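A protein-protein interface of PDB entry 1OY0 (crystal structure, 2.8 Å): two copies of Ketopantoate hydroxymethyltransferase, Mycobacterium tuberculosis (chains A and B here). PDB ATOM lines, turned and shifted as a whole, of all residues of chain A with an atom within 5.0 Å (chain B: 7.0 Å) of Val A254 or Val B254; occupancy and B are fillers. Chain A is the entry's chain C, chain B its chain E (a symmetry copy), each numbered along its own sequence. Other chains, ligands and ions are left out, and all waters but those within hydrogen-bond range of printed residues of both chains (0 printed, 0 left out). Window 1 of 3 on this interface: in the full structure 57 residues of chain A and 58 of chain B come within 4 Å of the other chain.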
ATOM      1  N   ALA A 237      18.888  13.525  -8.218  1.00  0.00           N
ATOM      2  CA  ALA A 237      20.056  14.038  -7.514  1.00  0.00           C
ATOM      3  C   ALA A 237      20.160  15.557  -7.475  1.00  0.00           C
ATOM      4  O   ALA A 237      21.243  16.098  -7.229  1.00  0.00           O
ATOM      5  CB  ALA A 237      21.318  13.448  -8.127  1.00  0.00           C
ATOM      6  N   GLY A 238      19.044  16.246  -7.706  1.00  0.00           N
ATOM      7  CA  GLY A 238      19.056  17.702  -7.686  1.00  0.00           C
ATOM      8  C   GLY A 238      20.197  18.270  -8.515  1.00  0.00           C
ATOM      9  O   GLY A 238      21.153  18.846  -7.982  1.00  0.00           O
ATOM     10  N   PHE A 239      20.096  18.102  -9.829  1.00  0.00           N
ATOM     11  CA  PHE A 239      21.127  18.572 -10.742  1.00  0.00           C
ATOM     12  C   PHE A 239      20.528  19.584 -11.719  1.00  0.00           C
ATOM     13  O   PHE A 239      21.249  20.270 -12.451  1.00  0.00           O
ATOM     14  CB  PHE A 239      21.694  17.389 -11.524  1.00  0.00           C
ATOM     15  CG  PHE A 239      23.061  17.627 -12.065  1.00  0.00           C
ATOM     16  CD1 PHE A 239      24.179  17.451 -11.254  1.00  0.00           C
ATOM     17  CD2 PHE A 239      23.244  18.026 -13.384  1.00  0.00           C
ATOM     18  CE1 PHE A 239      25.465  17.664 -11.747  1.00  0.00           C
ATOM     19  CE2 PHE A 239      24.529  18.245 -13.892  1.00  0.00           C
ATOM     20  CZ  PHE A 239      25.641  18.062 -13.072  1.00  0.00           C
ATOM     21  N   ALA A 252      19.411  14.120  -3.053  1.00  0.00           N
ATOM     22  CA  ALA A 252      20.667  14.843  -2.835  1.00  0.00           C
ATOM     23  C   ALA A 252      20.677  16.169  -3.579  1.00  0.00           C
ATOM     24  O   ALA A 252      19.695  16.542  -4.238  1.00  0.00           O
ATOM     25  CB  ALA A 252      21.864  13.994  -3.283  1.00  0.00           C
ATOM     26  N   ASP A 253      21.791  16.878  -3.450  1.00  0.00           N
ATOM     27  CA  ASP A 253      21.980  18.161  -4.110  1.00  0.00           C
ATOM     28  C   ASP A 253      23.321  18.082  -4.823  1.00  0.00           C
ATOM     29  O   ASP A 253      24.239  18.863  -4.545  1.00  0.00           O
ATOM     30  CB  ASP A 253      22.011  19.298  -3.093  1.00  0.00           C
ATOM     31  CG  ASP A 253      22.205  20.650  -3.741  1.00  0.00           C
ATOM     32  OD1 ASP A 253      22.680  21.578  -3.041  1.00  0.00           O
ATOM     33  OD2 ASP A 253      21.877  20.786  -4.946  1.00  0.00           O
ATOM     34  N   VAL A 254      23.431  17.113  -5.729  1.00  0.00           N
ATOM     35  CA  VAL A 254      24.652  16.910  -6.494  1.00  0.00           C
ATOM     36  C   VAL A 254      24.958  18.159  -7.325  1.00  0.00           C
ATOM     37  O   VAL A 254      26.125  18.500  -7.551  1.00  0.00           O
ATOM     38  CB  VAL A 254      24.513  15.690  -7.416  1.00  0.00           C
ATOM     39  CG1 VAL A 254      25.800  15.469  -8.183  1.00  0.00           C
ATOM     40  CG2 VAL A 254      24.182  14.464  -6.590  1.00  0.00           C
ATOM     41  N   GLY A 255      23.899  18.840  -7.759  1.00  0.00           N
ATOM     42  CA  GLY A 255      24.070  20.052  -8.536  1.00  0.00           C
ATOM     43  C   GLY A 255      24.751  21.104  -7.686  1.00  0.00           C
ATOM     44  O   GLY A 255      25.784  21.663  -8.073  1.00  0.00           O
ATOM     45  N   GLY A 256      24.168  21.369  -6.519  1.00  0.00           N
ATOM     46  CA  GLY A 256      24.731  22.353  -5.615  1.00  0.00           C
ATOM     47  C   GLY A 256      26.170  22.026  -5.279  1.00  0.00           C
ATOM     48  O   GLY A 256      27.039  22.902  -5.306  1.00  0.00           O
ATOM     49  N   GLU A 257      26.425  20.759  -4.970  1.00  0.00           N
ATOM     50  CA  GLU A 257      27.766  20.310  -4.624  1.00  0.00           C
ATOM     51  C   GLU A 257      28.738  20.688  -5.733  1.00  0.00           C
ATOM     52  O   GLU A 257      29.892  21.038  -5.471  1.00  0.00           O
ATOM     53  CB  GLU A 257      27.775  18.794  -4.421  1.00  0.00           C
ATOM     54  CG  GLU A 257      28.230  18.320  -3.034  1.00  0.00           C
ATOM     55  CD  GLU A 257      29.719  18.576  -2.755  1.00  0.00           C
ATOM     56  OE1 GLU A 257      30.117  19.759  -2.605  1.00  0.00           O
ATOM     57  OE2 GLU A 257      30.491  17.585  -2.687  1.00  0.00           O
ATOM     58  N   LEU A 258      28.264  20.627  -6.974  1.00  0.00           N
ATOM     59  CA  LEU A 258      29.105  20.965  -8.118  1.00  0.00           C
ATOM     60  C   LEU A 258      29.328  22.474  -8.199  1.00  0.00           C
ATOM     61  O   LEU A 258      30.378  22.936  -8.658  1.00  0.00           O
ATOM     62  CB  LEU A 258      28.472  20.449  -9.414  1.00  0.00           C
ATOM     63  CG  LEU A 258      29.302  20.569 -10.695  1.00  0.00           C
ATOM     64  CD1 LEU A 258      30.680  19.954 -10.496  1.00  0.00           C
ATOM     65  CD2 LEU A 258      28.562  19.871 -11.829  1.00  0.00           C
ATOM     66  N   ILE B  49      24.804  25.043 -14.341  1.00  0.00           N
ATOM     67  CA  ILE B  49      25.403  25.107 -13.019  1.00  0.00           C
ATOM     68  C   ILE B  49      26.657  25.969 -13.023  1.00  0.00           C
ATOM     69  O   ILE B  49      26.767  26.899 -12.230  1.00  0.00           O
ATOM     70  CB  ILE B  49      25.739  23.683 -12.495  1.00  0.00           C
ATOM     71  CG1 ILE B  49      24.440  22.941 -12.160  1.00  0.00           C
ATOM     72  CG2 ILE B  49      26.638  23.759 -11.269  1.00  0.00           C
ATOM     73  CD1 ILE B  49      24.637  21.494 -11.735  1.00  0.00           C
ATOM     74  N   TRP B 233      35.955  19.213 -15.804  1.00  0.00           N
ATOM     75  CA  TRP B 233      35.096  19.191 -14.625  1.00  0.00           C
ATOM     76  C   TRP B 233      34.924  17.825 -13.969  1.00  0.00           C
ATOM     77  O   TRP B 233      34.752  17.730 -12.751  1.00  0.00           O
ATOM     78  CB  TRP B 233      33.730  19.828 -14.925  1.00  0.00           C
ATOM     79  CG  TRP B 233      32.682  18.933 -15.496  1.00  0.00           C
ATOM     80  CD1 TRP B 233      32.261  18.890 -16.790  1.00  0.00           C
ATOM     81  CD2 TRP B 233      31.839  18.031 -14.774  1.00  0.00           C
ATOM     82  NE1 TRP B 233      31.199  18.030 -16.919  1.00  0.00           N
ATOM     83  CE2 TRP B 233      30.920  17.487 -15.695  1.00  0.00           C
ATOM     84  CE3 TRP B 233      31.771  17.630 -13.433  1.00  0.00           C
ATOM     85  CZ2 TRP B 233      29.936  16.560 -15.319  1.00  0.00           C
ATOM     86  CZ3 TRP B 233      30.795  16.706 -13.058  1.00  0.00           C
ATOM     87  CH2 TRP B 233      29.891  16.183 -14.000  1.00  0.00           C
ATOM     88  N   GLN B 234      34.987  16.768 -14.769  1.00  0.00           N
ATOM     89  CA  GLN B 234      34.854  15.414 -14.245  1.00  0.00           C
ATOM     90  C   GLN B 234      35.938  15.162 -13.195  1.00  0.00           C
ATOM     91  O   GLN B 234      35.676  14.555 -12.156  1.00  0.00           O
ATOM     92  CB  GLN B 234      35.009  14.400 -15.375  1.00  0.00           C
ATOM     93  CG  GLN B 234      34.527  14.915 -16.713  1.00  0.00           C
ATOM     94  CD  GLN B 234      33.053  15.132 -16.731  1.00  0.00           C
ATOM     95  OE1 GLN B 234      32.372  14.899 -15.735  1.00  0.00           O
ATOM     96  NE2 GLN B 234      32.539  15.573 -17.863  1.00  0.00           N
ATOM     97  N   MET B 236      37.847  17.663 -11.723  1.00  0.00           N
ATOM     98  CA  MET B 236      37.699  18.718 -10.737  1.00  0.00           C
ATOM     99  C   MET B 236      36.704  18.342  -9.636  1.00  0.00           C
ATOM    100  O   MET B 236      36.899  18.677  -8.464  1.00  0.00           O
ATOM    101  CB  MET B 236      37.260  20.008 -11.445  1.00  0.00           C
ATOM    102  CG  MET B 236      37.086  21.227 -10.547  1.00  0.00           C
ATOM    103  SD  MET B 236      35.546  21.206  -9.602  1.00  0.00           S
ATOM    104  CE  MET B 236      34.375  21.793 -10.860  1.00  0.00           C
ATOM    105  N   ALA B 237      35.643  17.634 -10.003  1.00  0.00           N
ATOM    106  CA  ALA B 237      34.636  17.255  -9.019  1.00  0.00           C
ATOM    107  C   ALA B 237      34.571  15.756  -8.708  1.00  0.00           C
ATOM    108  O   ALA B 237      33.564  15.275  -8.180  1.00  0.00           O
ATOM    109  CB  ALA B 237      33.278  17.745  -9.481  1.00  0.00           C
ATOM    110  N   GLY B 238      35.638  15.024  -9.029  1.00  0.00           N
ATOM    111  CA  GLY B 238      35.656  13.591  -8.773  1.00  0.00           C
ATOM    112  C   GLY B 238      34.399  12.909  -9.289  1.00  0.00           C
ATOM    113  O   GLY B 238      33.556  12.449  -8.508  1.00  0.00           O
ATOM    114  N   PHE B 239      34.273  12.846 -10.612  1.00  0.00           N
ATOM    115  CA  PHE B 239      33.103  12.242 -11.239  1.00  0.00           C
ATOM    116  C   PHE B 239      33.532  11.081 -12.109  1.00  0.00           C
ATOM    117  O   PHE B 239      32.709  10.286 -12.559  1.00  0.00           O
ATOM    118  CB  PHE B 239      32.383  13.272 -12.107  1.00  0.00           C
ATOM    119  CG  PHE B 239      30.933  12.966 -12.336  1.00  0.00           C
ATOM    120  CD1 PHE B 239      29.978  13.285 -11.371  1.00  0.00           C
ATOM    121  CD2 PHE B 239      30.516  12.368 -13.518  1.00  0.00           C
ATOM    122  CE1 PHE B 239      28.622  13.014 -11.583  1.00  0.00           C
ATOM    123  CE2 PHE B 239      29.160  12.090 -13.742  1.00  0.00           C
ATOM    124  CZ  PHE B 239      28.210  12.415 -12.771  1.00  0.00           C
ATOM    125  N   ARG B 250      41.299  17.506  -6.632  1.00  0.00           N
ATOM    126  CA  ARG B 250      39.942  17.009  -6.449  1.00  0.00           C
ATOM    127  C   ARG B 250      39.170  17.911  -5.481  1.00  0.00           C
ATOM    128  O   ARG B 250      39.307  17.785  -4.269  1.00  0.00           O
ATOM    129  CB  ARG B 250      40.025  15.580  -5.919  1.00  0.00           C
ATOM    130  CG  ARG B 250      38.857  14.685  -6.268  1.00  0.00           C
ATOM    131  CD  ARG B 250      39.298  13.225  -6.178  1.00  0.00           C
ATOM    132  NE  ARG B 250      38.196  12.297  -6.430  1.00  0.00           N
ATOM    133  CZ  ARG B 250      37.146  12.143  -5.624  1.00  0.00           C
ATOM    134  NH1 ARG B 250      37.056  12.861  -4.505  1.00  0.00           N
ATOM    135  NH2 ARG B 250      36.193  11.265  -5.933  1.00  0.00           N
ATOM    136  N   TYR B 251      38.361  18.819  -6.017  1.00  0.00           N
ATOM    137  CA  TYR B 251      37.591  19.743  -5.185  1.00  0.00           C
ATOM    138  C   TYR B 251      36.342  19.157  -4.558  1.00  0.00           C
ATOM    139  O   TYR B 251      35.618  19.859  -3.848  1.00  0.00           O
ATOM    140  CB  TYR B 251      37.188  20.985  -5.982  1.00  0.00           C
ATOM    141  CG  TYR B 251      38.318  21.951  -6.202  1.00  0.00           C
ATOM    142  CD1 TYR B 251      39.351  21.652  -7.093  1.00  0.00           C
ATOM    143  CD2 TYR B 251      38.376  23.159  -5.492  1.00  0.00           C
ATOM    144  CE1 TYR B 251      40.421  22.529  -7.276  1.00  0.00           C
ATOM    145  CE2 TYR B 251      39.440  24.046  -5.664  1.00  0.00           C
ATOM    146  CZ  TYR B 251      40.459  23.721  -6.561  1.00  0.00           C
ATOM    147  OH  TYR B 251      41.515  24.583  -6.749  1.00  0.00           O
ATOM    148  N   ALA B 252      36.077  17.882  -4.822  1.00  0.00           N
ATOM    149  CA  ALA B 252      34.900  17.222  -4.268  1.00  0.00           C
ATOM    150  C   ALA B 252      34.785  15.789  -4.766  1.00  0.00           C
ATOM    151  O   ALA B 252      35.642  15.305  -5.515  1.00  0.00           O
ATOM    152  CB  ALA B 252      33.635  17.999  -4.634  1.00  0.00           C
ATOM    153  N   ASP B 253      33.722  15.117  -4.329  1.00  0.00           N
ATOM    154  CA  ASP B 253      33.448  13.741  -4.724  1.00  0.00           C
ATOM    155  C   ASP B 253      32.005  13.705  -5.202  1.00  0.00           C
ATOM    156  O   ASP B 253      31.168  12.967  -4.671  1.00  0.00           O
ATOM    157  CB  ASP B 253      33.614  12.796  -3.537  1.00  0.00           C
ATOM    158  CG  ASP B 253      33.326  11.351  -3.902  1.00  0.00           C
ATOM    159  OD1 ASP B 253      33.010  10.560  -2.973  1.00  0.00           O
ATOM    160  OD2 ASP B 253      33.418  11.006  -5.113  1.00  0.00           O
ATOM    161  N   VAL B 254      31.713  14.531  -6.201  1.00  0.00           N
ATOM    162  CA  VAL B 254      30.373  14.611  -6.758  1.00  0.00           C
ATOM    163  C   VAL B 254      29.948  13.252  -7.296  1.00  0.00           C
ATOM    164  O   VAL B 254      28.772  12.888  -7.245  1.00  0.00           O
ATOM    165  CB  VAL B 254      30.314  15.658  -7.877  1.00  0.00           C
ATOM    166  CG1 VAL B 254      28.903  15.754  -8.428  1.00  0.00           C
ATOM    167  CG2 VAL B 254      30.759  17.003  -7.329  1.00  0.00           C
ATOM    168  N   GLY B 255      30.919  12.503  -7.807  1.00  0.00           N
ATOM    169  CA  GLY B 255      30.625  11.184  -8.325  1.00  0.00           C
ATOM    170  C   GLY B 255      30.133  10.290  -7.203  1.00  0.00           C
ATOM    171  O   GLY B 255      29.062   9.683  -7.296  1.00  0.00           O
ATOM    172  N   GLY B 256      30.921  10.213  -6.133  1.00  0.00           N
ATOM    173  CA  GLY B 256      30.544   9.392  -5.002  1.00  0.00           C
ATOM    174  C   GLY B 256      29.184   9.792  -4.469  1.00  0.00           C
ATOM    175  O   GLY B 256      28.342   8.932  -4.202  1.00  0.00           O
ATOM    176  N   GLU B 257      28.967  11.096  -4.317  1.00  0.00           N
ATOM    177  CA  GLU B 257      27.702  11.608  -3.809  1.00  0.00           C
ATOM    178  C   GLU B 257      26.550  11.068  -4.647  1.00  0.00           C
ATOM    179  O   GLU B 257      25.462  10.797  -4.127  1.00  0.00           O
ATOM    180  CB  GLU B 257      27.708  13.135  -3.854  1.00  0.00           C
ATOM    181  CG  GLU B 257      27.501  13.830  -2.503  1.00  0.00           C
ATOM    182  CD  GLU B 257      26.093  13.642  -1.940  1.00  0.00           C
ATOM    183  OE1 GLU B 257      25.747  12.500  -1.534  1.00  0.00           O
ATOM    184  OE2 GLU B 257      25.336  14.643  -1.911  1.00  0.00           O
ATOM    185  N   LEU B 258      26.799  10.904  -5.945  1.00  0.00           N
ATOM    186  CA  LEU B 258      25.778  10.396  -6.853  1.00  0.00           C
ATOM    187  C   LEU B 258      25.573   8.901  -6.648  1.00  0.00           C
ATOM    188  O   LEU B 258      24.472   8.386  -6.823  1.00  0.00           O
ATOM    189  CB  LEU B 258      26.165  10.681  -8.307  1.00  0.00           C
ATOM    190  CG  LEU B 258      25.114  10.369  -9.381  1.00  0.00           C
ATOM    191  CD1 LEU B 258      23.774  11.027  -9.037  1.00  0.00           C
ATOM    192  CD2 LEU B 258      25.625  10.862 -10.732  1.00  0.00           C
ATOM    193  N   ARG B 259      26.631   8.203  -6.263  1.00  0.00           N
ATOM    194  CA  ARG B 259      26.509   6.770  -6.028  1.00  0.00           C
ATOM    195  C   ARG B 259      25.531   6.448  -4.902  1.00  0.00           C
ATOM    196  O   ARG B 259      24.666   5.592  -5.079  1.00  0.00           O
ATOM    197  CB  ARG B 259      27.866   6.160  -5.720  1.00  0.00           C
ATOM    198  CG  ARG B 259      28.783   6.188  -6.901  1.00  0.00           C
ATOM    199  CD  ARG B 259      30.103   5.614  -6.525  1.00  0.00           C
ATOM    200  NE  ARG B 259      29.888   4.276  -6.019  1.00  0.00           N
ATOM    201  CZ  ARG B 259      30.833   3.519  -5.481  1.00  0.00           C
ATOM    202  NH1 ARG B 259      32.086   3.955  -5.371  1.00  0.00           N
ATOM    203  NH2 ARG B 259      30.511   2.313  -5.041  1.00  0.00           N
ATOM    204  N   ALA B 261      23.171   8.456  -3.593  1.00  0.00           N
ATOM    205  CA  ALA B 261      21.864   8.937  -4.038  1.00  0.00           C
ATOM    206  C   ALA B 261      21.164   7.829  -4.815  1.00  0.00           C
ATOM    207  O   ALA B 261      19.984   7.551  -4.606  1.00  0.00           O
ATOM    208  CB  ALA B 261      22.030  10.174  -4.915  1.00  0.00           C
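O of Gly A238 sits at hydrogen-bond distance from N of Gly A255 (2.8 Å).
O of Ala A237 lies within hydrogen-bond range of N of Val A254, at 2.8 Å.
O of Ala B237 sits at hydrogen-bond distance from N of Val B254 (2.8 Å).
The indole nitrogen of Trp B233 sits close to the side-chain amide nitrogen of Gln B234 (3.0 Å).
The backbone carbonyl oxygen (O) of Ala B252 is in hydrogen-bond range of the guanidinium group (NH1) of Arg B250 (3.0 Å).
Printed residues of chain B within 4 Å of Ala A237: Leu B258.
Val A254 touches just one residue of chain B: Val B254.
Gln B234 touches none of the printed residues of chain A.
Of the printed residues of chain A, Ala B237 touches Leu A258.
Of chain A, only Val A254 (3.1 Å) comes within 4 Å of Val B254.
Gly B256 touches none of the printed residues of chain A.
Of the printed residues of chain A, Glu B257 touches Ala A252 (3.8 Å).
The nearest residue of chain B that does not touch Val A254 is Leu B258 (4.2 Å).
Hydrophobic or aromatic side chains of chain A within 4 Å of the printed part of chain B: Ala A237, Phe A239, Ala A252, Val A254 and Leu A258.
Among the printed residues, 8 pairs touch across the chains.
Among the printed residues, merely in contact across the chains: Val A254 with Val B254 (3.1 Å), Gly A255 with Ile B49 (3.6 Å), Leu A258 with Ala B237 (3.6 Å), Ala A237 with Leu B258 (3.6 Å), Phe A239 with Ile B49 (3.7 Å), Glu A257 with Ala B252 (3.7 Å), Ala A252 with Glu B257 (3.8 Å) and Leu A258 with Trp B233 (3.9 Å).
Ala A237 touches Leu B258, and with the chains exchanged Leu A258 touches Ala B237.
Ala A252 touches Glu B257, and with the chains exchanged Glu A257 touches Ala B252.
Val A254 touches its own counterpart, Val B254.
10 positions are printed for both chains.
Of the 8 pairs that touch across the chains among the printed residues, 5 have their exchanged pair printed and touching as well.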
